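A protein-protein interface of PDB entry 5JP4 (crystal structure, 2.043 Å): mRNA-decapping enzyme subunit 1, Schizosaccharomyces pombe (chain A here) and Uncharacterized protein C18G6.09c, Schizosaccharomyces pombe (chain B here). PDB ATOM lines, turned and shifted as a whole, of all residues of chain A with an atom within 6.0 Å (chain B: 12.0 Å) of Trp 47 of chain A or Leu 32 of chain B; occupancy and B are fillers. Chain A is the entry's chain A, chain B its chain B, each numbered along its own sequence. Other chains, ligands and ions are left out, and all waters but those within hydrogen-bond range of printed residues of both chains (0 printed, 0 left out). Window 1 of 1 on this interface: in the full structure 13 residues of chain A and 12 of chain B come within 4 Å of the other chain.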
ATOM      1  N   TYR A  38      -3.709 -17.566   9.739  1.00  0.00           N
ATOM      2  CA  TYR A  38      -4.045 -18.757   8.976  1.00  0.00           C
ATOM      3  C   TYR A  38      -3.898 -19.980   9.867  1.00  0.00           C
ATOM      4  O   TYR A  38      -3.123 -19.984  10.832  1.00  0.00           O
ATOM      5  CB  TYR A  38      -3.129 -18.922   7.753  1.00  0.00           C
ATOM      6  CG  TYR A  38      -3.094 -17.728   6.835  1.00  0.00           C
ATOM      7  CD1 TYR A  38      -2.423 -16.564   7.203  1.00  0.00           C
ATOM      8  CD2 TYR A  38      -3.718 -17.765   5.589  1.00  0.00           C
ATOM      9  CE1 TYR A  38      -2.386 -15.466   6.367  1.00  0.00           C
ATOM     10  CE2 TYR A  38      -3.693 -16.679   4.753  1.00  0.00           C
ATOM     11  CZ  TYR A  38      -3.015 -15.527   5.142  1.00  0.00           C
ATOM     12  OH  TYR A  38      -2.969 -14.432   4.302  1.00  0.00           O
ATOM     13  N   GLN A  39      -4.609 -21.039   9.495  1.00  0.00           N
ATOM     14  CA  GLN A  39      -4.597 -22.293  10.222  1.00  0.00           C
ATOM     15  C   GLN A  39      -4.326 -23.430   9.247  1.00  0.00           C
ATOM     16  O   GLN A  39      -4.885 -23.456   8.147  1.00  0.00           O
ATOM     17  CB  GLN A  39      -5.951 -22.517  10.925  1.00  0.00           C
ATOM     18  CG  GLN A  39      -6.033 -23.758  11.774  1.00  0.00           C
ATOM     19  CD  GLN A  39      -7.198 -23.685  12.749  1.00  0.00           C
ATOM     20  OE1 GLN A  39      -7.089 -24.115  13.898  1.00  0.00           O
ATOM     21  NE2 GLN A  39      -8.316 -23.106  12.294  1.00  0.00           N
ATOM     22  N   PHE A  40      -3.498 -24.386   9.652  1.00  0.00           N
ATOM     23  CA  PHE A  40      -3.185 -25.516   8.782  1.00  0.00           C
ATOM     24  C   PHE A  40      -4.117 -26.673   9.103  1.00  0.00           C
ATOM     25  O   PHE A  40      -4.099 -27.201  10.219  1.00  0.00           O
ATOM     26  CB  PHE A  40      -1.725 -25.943   8.919  1.00  0.00           C
ATOM     27  CG  PHE A  40      -1.316 -27.027   7.957  1.00  0.00           C
ATOM     28  CD1 PHE A  40      -1.170 -26.749   6.606  1.00  0.00           C
ATOM     29  CD2 PHE A  40      -1.053 -28.305   8.404  1.00  0.00           C
ATOM     30  CE1 PHE A  40      -0.799 -27.741   5.714  1.00  0.00           C
ATOM     31  CE2 PHE A  40      -0.672 -29.302   7.523  1.00  0.00           C
ATOM     32  CZ  PHE A  40      -0.546 -29.015   6.170  1.00  0.00           C
ATOM     33  N   ASP A  41      -4.930 -27.061   8.125  1.00  0.00           N
ATOM     34  CA  ASP A  41      -5.823 -28.206   8.266  1.00  0.00           C
ATOM     35  C   ASP A  41      -5.066 -29.436   7.784  1.00  0.00           C
ATOM     36  O   ASP A  41      -5.009 -29.719   6.585  1.00  0.00           O
ATOM     37  CB  ASP A  41      -7.111 -27.998   7.481  1.00  0.00           C
ATOM     38  CG  ASP A  41      -8.132 -29.068   7.771  1.00  0.00           C
ATOM     39  OD1 ASP A  41      -8.726 -29.046   8.871  1.00  0.00           O
ATOM     40  OD2 ASP A  41      -8.335 -29.930   6.899  1.00  0.00           O
ATOM     41  N   GLN A  45      -4.294 -31.278   4.610  1.00  0.00           N
ATOM     42  CA  GLN A  45      -3.019 -30.765   4.100  1.00  0.00           C
ATOM     43  C   GLN A  45      -3.183 -29.429   3.388  1.00  0.00           C
ATOM     44  O   GLN A  45      -2.490 -29.147   2.409  1.00  0.00           O
ATOM     45  CB  GLN A  45      -2.340 -31.769   3.166  1.00  0.00           C
ATOM     46  CG  GLN A  45      -1.817 -32.983   3.869  1.00  0.00           C
ATOM     47  CD  GLN A  45      -0.875 -32.619   4.987  1.00  0.00           C
ATOM     48  OE1 GLN A  45      -1.166 -32.873   6.151  1.00  0.00           O
ATOM     49  NE2 GLN A  45       0.254 -32.009   4.644  1.00  0.00           N
ATOM     50  N   LYS A  46      -4.106 -28.600   3.862  1.00  0.00           N
ATOM     51  CA  LYS A  46      -4.354 -27.309   3.247  1.00  0.00           C
ATOM     52  C   LYS A  46      -4.345 -26.240   4.325  1.00  0.00           C
ATOM     53  O   LYS A  46      -4.819 -26.468   5.445  1.00  0.00           O
ATOM     54  CB  LYS A  46      -5.689 -27.286   2.487  1.00  0.00           C
ATOM     55  N   TRP A  47      -3.775 -25.088   3.990  1.00  0.00           N
ATOM     56  CA  TRP A  47      -3.938 -23.906   4.819  1.00  0.00           C
ATOM     57  C   TRP A  47      -5.326 -23.327   4.605  1.00  0.00           C
ATOM     58  O   TRP A  47      -5.873 -23.383   3.501  1.00  0.00           O
ATOM     59  CB  TRP A  47      -2.883 -22.854   4.482  1.00  0.00           C
ATOM     60  CG  TRP A  47      -1.517 -23.150   5.021  1.00  0.00           C
ATOM     61  CD1 TRP A  47      -0.467 -23.696   4.341  1.00  0.00           C
ATOM     62  CD2 TRP A  47      -1.050 -22.899   6.349  1.00  0.00           C
ATOM     63  NE1 TRP A  47       0.625 -23.814   5.171  1.00  0.00           N
ATOM     64  CE2 TRP A  47       0.296 -23.324   6.406  1.00  0.00           C
ATOM     65  CE3 TRP A  47      -1.643 -22.357   7.503  1.00  0.00           C
ATOM     66  CZ2 TRP A  47       1.065 -23.227   7.570  1.00  0.00           C
ATOM     67  CZ3 TRP A  47      -0.888 -22.261   8.650  1.00  0.00           C
ATOM     68  CH2 TRP A  47       0.465 -22.689   8.676  1.00  0.00           C
ATOM     69  N   LEU A  48      -5.904 -22.794   5.674  1.00  0.00           N
ATOM     70  CA  LEU A  48      -7.138 -22.031   5.598  1.00  0.00           C
ATOM     71  C   LEU A  48      -6.862 -20.653   6.157  1.00  0.00           C
ATOM     72  O   LEU A  48      -6.112 -20.517   7.132  1.00  0.00           O
ATOM     73  CB  LEU A  48      -8.284 -22.711   6.380  1.00  0.00           C
ATOM     74  CG  LEU A  48      -8.527 -24.191   6.075  1.00  0.00           C
ATOM     75  CD1 LEU A  48      -9.341 -24.875   7.189  1.00  0.00           C
ATOM     76  CD2 LEU A  48      -9.243 -24.347   4.741  1.00  0.00           C
ATOM     77  N   LYS A  49      -7.437 -19.632   5.531  1.00  0.00           N
ATOM     78  CA  LYS A  49      -7.375 -18.294   6.095  1.00  0.00           C
ATOM     79  C   LYS A  49      -8.532 -18.127   7.072  1.00  0.00           C
ATOM     80  O   LYS A  49      -9.673 -18.471   6.753  1.00  0.00           O
ATOM     81  CB  LYS A  49      -7.430 -17.207   5.021  1.00  0.00           C
ATOM     82  CG  LYS A  49      -7.216 -15.808   5.622  1.00  0.00           C
ATOM     83  CD  LYS A  49      -7.553 -14.692   4.655  1.00  0.00           C
ATOM     84  CE  LYS A  49      -6.565 -14.635   3.505  1.00  0.00           C
ATOM     85  NZ  LYS A  49      -6.636 -13.337   2.762  1.00  0.00           N
ATOM     86  N   TYR A  95       6.010 -15.576   6.240  1.00  0.00           N
ATOM     87  CA  TYR A  95       5.072 -15.945   7.293  1.00  0.00           C
ATOM     88  C   TYR A  95       5.815 -16.347   8.561  1.00  0.00           C
ATOM     89  O   TYR A  95       6.911 -16.909   8.506  1.00  0.00           O
ATOM     90  CB  TYR A  95       4.167 -17.104   6.814  1.00  0.00           C
ATOM     91  CG  TYR A  95       3.459 -16.769   5.525  1.00  0.00           C
ATOM     92  CD1 TYR A  95       2.295 -16.016   5.535  1.00  0.00           C
ATOM     93  CD2 TYR A  95       3.997 -17.147   4.292  1.00  0.00           C
ATOM     94  CE1 TYR A  95       1.663 -15.677   4.376  1.00  0.00           C
ATOM     95  CE2 TYR A  95       3.361 -16.811   3.108  1.00  0.00           C
ATOM     96  CZ  TYR A  95       2.194 -16.078   3.166  1.00  0.00           C
ATOM     97  OH  TYR A  95       1.556 -15.729   2.010  1.00  0.00           O
ATOM     98  N   ILE A  97       5.387 -19.054  11.263  1.00  0.00           N
ATOM     99  CA  ILE A  97       4.708 -20.326  11.471  1.00  0.00           C
ATOM    100  C   ILE A  97       4.895 -20.724  12.927  1.00  0.00           C
ATOM    101  O   ILE A  97       6.027 -20.791  13.430  1.00  0.00           O
ATOM    102  CB  ILE A  97       5.236 -21.413  10.517  1.00  0.00           C
ATOM    103  CG1 ILE A  97       4.434 -21.428   9.215  1.00  0.00           C
ATOM    104  CG2 ILE A  97       5.085 -22.799  11.131  1.00  0.00           C
ATOM    105  CD1 ILE A  97       4.594 -20.238   8.375  1.00  0.00           C
ATOM    106  N   VAL A 105      -0.815 -26.139  13.905  1.00  0.00           N
ATOM    107  CA  VAL A 105       0.009 -25.129  13.244  1.00  0.00           C
ATOM    108  C   VAL A 105      -0.875 -23.957  12.849  1.00  0.00           C
ATOM    109  O   VAL A 105      -1.918 -24.152  12.209  1.00  0.00           O
ATOM    110  CB  VAL A 105       0.722 -25.692  11.995  1.00  0.00           C
ATOM    111  CG1 VAL A 105       1.713 -24.652  11.421  1.00  0.00           C
ATOM    112  CG2 VAL A 105       1.427 -26.977  12.309  1.00  0.00           C
ATOM    113  N   VAL A 106      -0.482 -22.750  13.260  1.00  0.00           N
ATOM    114  CA  VAL A 106      -1.046 -21.511  12.751  1.00  0.00           C
ATOM    115  C   VAL A 106       0.059 -20.731  12.047  1.00  0.00           C
ATOM    116  O   VAL A 106       1.255 -20.961  12.265  1.00  0.00           O
ATOM    117  CB  VAL A 106      -1.716 -20.655  13.850  1.00  0.00           C
ATOM    118  CG1 VAL A 106      -2.841 -21.465  14.544  1.00  0.00           C
ATOM    119  CG2 VAL A 106      -0.697 -20.153  14.855  1.00  0.00           C
ATOM    120  N   GLY A 107      -0.362 -19.830  11.166  1.00  0.00           N
ATOM    121  CA  GLY A 107       0.564 -18.981  10.427  1.00  0.00           C
ATOM    122  C   GLY A 107       0.097 -17.549  10.489  1.00  0.00           C
ATOM    123  O   GLY A 107      -1.106 -17.269  10.486  1.00  0.00           O
ATOM    124  N   LEU A 108       1.058 -16.631  10.584  1.00  0.00           N
ATOM    125  CA  LEU A 108       0.777 -15.214  10.729  1.00  0.00           C
ATOM    126  C   LEU A 108       1.412 -14.469   9.574  1.00  0.00           C
ATOM    127  O   LEU A 108       2.595 -14.673   9.266  1.00  0.00           O
ATOM    128  CB  LEU A 108       1.316 -14.649  12.045  1.00  0.00           C
ATOM    129  CG  LEU A 108       0.903 -15.372  13.323  1.00  0.00           C
ATOM    130  CD1 LEU A 108       1.611 -14.720  14.467  1.00  0.00           C
ATOM    131  CD2 LEU A 108      -0.612 -15.358  13.527  1.00  0.00           C
ATOM    132  N   MET B   3       9.911 -30.716  11.987  1.00  0.00           N
ATOM    133  CA  MET B   3       9.194 -30.398  10.762  1.00  0.00           C
ATOM    134  C   MET B   3      10.157 -29.948   9.673  1.00  0.00           C
ATOM    135  O   MET B   3      11.372 -29.855   9.872  1.00  0.00           O
ATOM    136  CB  MET B   3       8.144 -29.303  10.979  1.00  0.00           C
ATOM    137  CG  MET B   3       7.324 -29.401  12.240  1.00  0.00           C
ATOM    138  SD  MET B   3       6.851 -27.747  12.790  1.00  0.00           S
ATOM    139  CE  MET B   3       6.200 -27.066  11.286  1.00  0.00           C
ATOM    140  N   SER B   4       9.577 -29.652   8.513  1.00  0.00           N
ATOM    141  CA  SER B   4      10.254 -28.976   7.412  1.00  0.00           C
ATOM    142  C   SER B   4       9.176 -28.431   6.487  1.00  0.00           C
ATOM    143  O   SER B   4       7.982 -28.647   6.707  1.00  0.00           O
ATOM    144  CB  SER B   4      11.219 -29.913   6.680  1.00  0.00           C
ATOM    145  OG  SER B   4      10.516 -30.777   5.800  1.00  0.00           O
ATOM    146  N   PHE B   5       9.598 -27.718   5.449  1.00  0.00           N
ATOM    147  CA  PHE B   5       8.643 -27.038   4.576  1.00  0.00           C
ATOM    148  C   PHE B   5       8.995 -27.205   3.100  1.00  0.00           C
ATOM    149  O   PHE B   5       8.164 -26.959   2.224  1.00  0.00           O
ATOM    150  CB  PHE B   5       8.565 -25.546   4.934  1.00  0.00           C
ATOM    151  CG  PHE B   5       8.314 -25.279   6.399  1.00  0.00           C
ATOM    152  CD1 PHE B   5       9.370 -25.190   7.295  1.00  0.00           C
ATOM    153  CD2 PHE B   5       7.023 -25.119   6.877  1.00  0.00           C
ATOM    154  CE1 PHE B   5       9.145 -24.947   8.641  1.00  0.00           C
ATOM    155  CE2 PHE B   5       6.790 -24.876   8.218  1.00  0.00           C
ATOM    156  CZ  PHE B   5       7.851 -24.791   9.102  1.00  0.00           C
ATOM    157  N   HIS B  25      -5.701  -6.212   2.503  1.00  0.00           N
ATOM    158  CA  HIS B  25      -5.602  -7.390   1.653  1.00  0.00           C
ATOM    159  C   HIS B  25      -4.422  -8.270   2.066  1.00  0.00           C
ATOM    160  O   HIS B  25      -3.268  -7.832   2.038  1.00  0.00           O
ATOM    161  CB  HIS B  25      -5.467  -6.977   0.188  1.00  0.00           C
ATOM    162  N   SER B  26      -4.717  -9.522   2.454  1.00  0.00           N
ATOM    163  CA  SER B  26      -3.724 -10.502   2.898  1.00  0.00           C
ATOM    164  C   SER B  26      -3.589 -11.634   1.878  1.00  0.00           C
ATOM    165  O   SER B  26      -4.527 -11.906   1.123  1.00  0.00           O
ATOM    166  CB  SER B  26      -4.111 -11.078   4.270  1.00  0.00           C
ATOM    167  OG  SER B  26      -5.436 -11.580   4.262  1.00  0.00           O
ATOM    168  N   PRO B  27      -2.438 -12.309   1.824  1.00  0.00           N
ATOM    169  CA  PRO B  27      -2.247 -13.369   0.825  1.00  0.00           C
ATOM    170  C   PRO B  27      -3.274 -14.485   0.955  1.00  0.00           C
ATOM    171  O   PRO B  27      -3.781 -14.777   2.042  1.00  0.00           O
ATOM    172  CB  PRO B  27      -0.839 -13.897   1.126  1.00  0.00           C
ATOM    173  CG  PRO B  27      -0.161 -12.804   1.846  1.00  0.00           C
ATOM    174  CD  PRO B  27      -1.222 -12.084   2.614  1.00  0.00           C
ATOM    175  N   ALA B  28      -3.566 -15.127  -0.175  1.00  0.00           N
ATOM    176  CA  ALA B  28      -4.425 -16.302  -0.162  1.00  0.00           C
ATOM    177  C   ALA B  28      -3.731 -17.451   0.559  1.00  0.00           C
ATOM    178  O   ALA B  28      -2.507 -17.604   0.491  1.00  0.00           O
ATOM    179  CB  ALA B  28      -4.788 -16.715  -1.585  1.00  0.00           C
ATOM    180  N   ALA B  29      -4.527 -18.270   1.254  1.00  0.00           N
ATOM    181  CA  ALA B  29      -3.945 -19.333   2.070  1.00  0.00           C
ATOM    182  C   ALA B  29      -3.065 -20.268   1.250  1.00  0.00           C
ATOM    183  O   ALA B  29      -2.134 -20.873   1.799  1.00  0.00           O
ATOM    184  CB  ALA B  29      -5.048 -20.120   2.782  1.00  0.00           C
ATOM    185  N   SER B  30      -3.310 -20.362  -0.059  1.00  0.00           N
ATOM    186  CA  SER B  30      -2.495 -21.208  -0.920  1.00  0.00           C
ATOM    187  C   SER B  30      -1.045 -20.742  -1.016  1.00  0.00           C
ATOM    188  O   SER B  30      -0.190 -21.533  -1.423  1.00  0.00           O
ATOM    189  CB  SER B  30      -3.115 -21.273  -2.317  1.00  0.00           C
ATOM    190  OG  SER B  30      -3.237 -19.973  -2.867  1.00  0.00           O
ATOM    191  N   ASN B  31      -0.738 -19.493  -0.643  1.00  0.00           N
ATOM    192  CA  ASN B  31       0.628 -18.985  -0.739  1.00  0.00           C
ATOM    193  C   ASN B  31       1.510 -19.433   0.419  1.00  0.00           C
ATOM    194  O   ASN B  31       2.737 -19.308   0.329  1.00  0.00           O
ATOM    195  CB  ASN B  31       0.623 -17.456  -0.798  1.00  0.00           C
ATOM    196  CG  ASN B  31      -0.194 -16.917  -1.953  1.00  0.00           C
ATOM    197  OD1 ASN B  31      -1.078 -16.087  -1.764  1.00  0.00           O
ATOM    198  ND2 ASN B  31       0.103 -17.380  -3.155  1.00  0.00           N
ATOM    199  N   LEU B  32       0.922 -19.945   1.504  1.00  0.00           N
ATOM    200  CA  LEU B  32       1.700 -20.300   2.687  1.00  0.00           C
ATOM    201  C   LEU B  32       2.475 -21.596   2.453  1.00  0.00           C
ATOM    202  O   LEU B  32       1.994 -22.497   1.757  1.00  0.00           O
ATOM    203  CB  LEU B  32       0.790 -20.460   3.909  1.00  0.00           C
ATOM    204  CG  LEU B  32       0.451 -19.143   4.616  1.00  0.00           C
ATOM    205  CD1 LEU B  32      -0.689 -18.417   3.918  1.00  0.00           C
ATOM    206  CD2 LEU B  32       0.118 -19.386   6.097  1.00  0.00           C
ATOM    207  N   PRO B  33       3.673 -21.719   3.018  1.00  0.00           N
ATOM    208  CA  PRO B  33       4.464 -22.941   2.828  1.00  0.00           C
ATOM    209  C   PRO B  33       3.874 -24.082   3.630  1.00  0.00           C
ATOM    210  O   PRO B  33       3.304 -23.884   4.702  1.00  0.00           O
ATOM    211  CB  PRO B  33       5.850 -22.570   3.371  1.00  0.00           C
ATOM    212  CG  PRO B  33       5.617 -21.375   4.219  1.00  0.00           C
ATOM    213  CD  PRO B  33       4.401 -20.679   3.746  1.00  0.00           C
ATOM    214  N   ILE B  34       4.033 -25.297   3.126  1.00  0.00           N
ATOM    215  CA  ILE B  34       3.362 -26.466   3.681  1.00  0.00           C
ATOM    216  C   ILE B  34       4.265 -27.077   4.749  1.00  0.00           C
ATOM    217  O   ILE B  34       5.396 -27.480   4.423  1.00  0.00           O
ATOM    218  CB  ILE B  34       3.024 -27.497   2.603  1.00  0.00           C
ATOM    219  CG1 ILE B  34       2.366 -26.801   1.415  1.00  0.00           C
ATOM    220  CG2 ILE B  34       2.116 -28.575   3.190  1.00  0.00           C
ATOM    221  CD1 ILE B  34       0.978 -26.300   1.700  1.00  0.00           C
ATOM    222  N   PRO B  35       3.827 -27.170   6.001  1.00  0.00           N
ATOM    223  CA  PRO B  35       4.618 -27.886   7.008  1.00  0.00           C
ATOM    224  C   PRO B  35       4.525 -29.392   6.805  1.00  0.00           C
ATOM    225  O   PRO B  35       3.480 -29.923   6.418  1.00  0.00           O
ATOM    226  CB  PRO B  35       3.974 -27.461   8.330  1.00  0.00           C
ATOM    227  CG  PRO B  35       2.541 -27.169   7.965  1.00  0.00           C
ATOM    228  CD  PRO B  35       2.589 -26.594   6.566  1.00  0.00           C
ATOM    229  N   THR B  36       5.639 -30.079   7.061  1.00  0.00           N
ATOM    230  CA  THR B  36       5.728 -31.530   6.925  1.00  0.00           C
ATOM    231  C   THR B  36       6.288 -32.112   8.215  1.00  0.00           C
ATOM    232  O   THR B  36       7.353 -31.690   8.672  1.00  0.00           O
ATOM    233  CB  THR B  36       6.621 -31.934   5.739  1.00  0.00           C
ATOM    234  OG1 THR B  36       6.483 -30.982   4.674  1.00  0.00           O
ATOM    235  CG2 THR B  36       6.240 -33.320   5.232  1.00  0.00           C
ATOM    236  N   PHE B  37       5.584 -33.074   8.799  1.00  0.00           N
ATOM    237  CA  PHE B  37       6.006 -33.688  10.050  1.00  0.00           C
ATOM    238  C   PHE B  37       6.667 -35.030   9.771  1.00  0.00           C
ATOM    239  O   PHE B  37       6.170 -35.826   8.969  1.00  0.00           O
ATOM    240  CB  PHE B  37       4.818 -33.856  11.006  1.00  0.00           C
ATOM    241  CG  PHE B  37       4.261 -32.552  11.517  1.00  0.00           C
ATOM    242  CD1 PHE B  37       4.854 -31.904  12.595  1.00  0.00           C
ATOM    243  CD2 PHE B  37       3.160 -31.965  10.916  1.00  0.00           C
ATOM    244  CE1 PHE B  37       4.358 -30.700  13.070  1.00  0.00           C
ATOM    245  CE2 PHE B  37       2.661 -30.754  11.384  1.00  0.00           C
ATOM    246  CZ  PHE B  37       3.268 -30.123  12.462  1.00  0.00           C
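Of chain B, only Ser 26 (3.5 Å), Pro 27 (2.4 Å), Ala 29 (3.8 Å) and Leu 32 (3.5 Å) come within 4 Å of Tyr 38 of chain A. Phe 40 of chain A touches two residues of chain B. No residue of chain B comes within 4 Å of Asp 41 of chain A. No residue of chain B comes within 4 Å of Lys 46 of chain A. Printed residues of chain B within 4 Å of Trp 47 of chain A: Ala 29, Leu 32, Pro 33, Ile 34 and Pro 35. Leu 48 of chain A touches just one residue of chain B: Ala 29 (3.9 Å). Of the printed residues of chain B, Tyr 95 of chain A touches Pro 27, Asn 31, Leu 32 and Pro 33. Val 105 of chain A touches one residue of chain B. No residue of chain B comes within 4 Å of Val 106 of chain A. No residue of chain B comes within 4 Å of Gly 107 of chain A. Met 3 of chain B touches none of the printed residues of chain A. Printed residues of chain A within 4 Å of Ala 29 of chain B: Tyr 38 (3.8 Å), Trp 47 (3.4 Å), Leu 48 (3.9 Å) and Lys 49 (3.7 Å). Printed residues of chain A within 4 Å of Pro 33 of chain B: Trp 47 (2.7 Å) and Tyr 95 (3.6 Å). Printed residues of chain A within 4 Å of Ile 34 of chain B: Phe 40 and Trp 47. Of the printed residues of chain A, Pro 35 of chain B touches Phe 40 and Trp 47. The nearest residue of chain A that does not touch Leu 32 of chain B is Gly 107 of chain A (4.4 Å). The nearest printed residue of chain A that does not touch Phe 5 of chain B is Trp 47 of chain A (6.0 Å).
CD2 of Tyr 38 of chain A touches CD1 of Leu 32 of chain B, 3.5 Å away. CE1 of Phe 40 of chain A touches CG2 of Ile 34 of chain B (3.9 Å). Leu 32 of chain B touches Trp 47 of chain A. Pro 35 of chain B touches Trp 47 of chain A (CD to NE1, 3.7 Å). C of Leu 48 of chain A touches CB of Ala 29 of chain B, at 3.9 Å. Ala 29 of chain B touches Lys 49 of chain A. CB of Asn 31 of chain B touches OH of Tyr 95 of chain A, 3.4 Å away. CD1 of Leu 32 of chain B touches CE1 of Tyr 95 of chain A, 3.6 Å away. Tyr 95 of chain A touches Pro 33 of chain B (CD2 to CD, 3.6 Å). Val 105 of chain A touches Phe 37 of chain B (CG2 to CZ, 3.6 Å).
The backbone carbonyl oxygen (O) of Pro 27 of chain B is in hydrogen-bond range of the side-chain hydroxyl (OH) of Tyr 38 of chain A. The backbone carbonyl oxygen of Pro 33 of chain B lies within hydrogen-bond range of the indole nitrogen of Trp 47 of chain A, at 2.7 Å. The side-chain amino group of Lys 49 of chain A lies within hydrogen-bond range of the side-chain hydroxyl of Ser 26 of chain B, at 2.6 Å. The side-chain amino group (NZ) of Lys 49 of chain A sits close to the backbone carbonyl oxygen (O) of Pro 27 of chain B (3.3 Å).
The backbone carbonyl oxygen (O) of Gly 107 of chain A sits at hydrogen-bond distance from the backbone NH (N) of Tyr 38 of chain A (2.7 Å). The backbone carbonyl oxygen of Gln 39 of chain A sits at hydrogen-bond distance from the backbone NH of Leu 48 of chain A (2.8 Å). The backbone NH (N) of Phe 40 of chain A sits at hydrogen-bond distance from the backbone carbonyl oxygen (O) of Val 105 of chain A (3.0 Å). OD1 of Asn 31 of chain B lies close to O of Ala 28 of chain B, 3.1 Å away.
Of the 16 printed residues of chain B, 10 touch a printed residue of chain A. Hydrophobic or aromatic side chains of chain B that line the printed part of chain A: Phe 5, Pro 27, Ala 29, Leu 32, Pro 33, Ile 34, Pro 35 and Phe 37. Of the 15 printed residues of chain A, 8 touch a printed residue of chain B. Hydrophobic or aromatic side chains of chain A within 4 Å of the printed part of chain B: Tyr 38, Phe 40, Trp 47, Tyr 95, Ile 97 and Val 105. Along chain A the printed residues that touch a printed residue of chain B span positions 38 to 105. Among the printed residues, no Asp or Glu carboxylate lies within 4 Å of a Lys or Arg side-chain nitrogen of the other chain.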
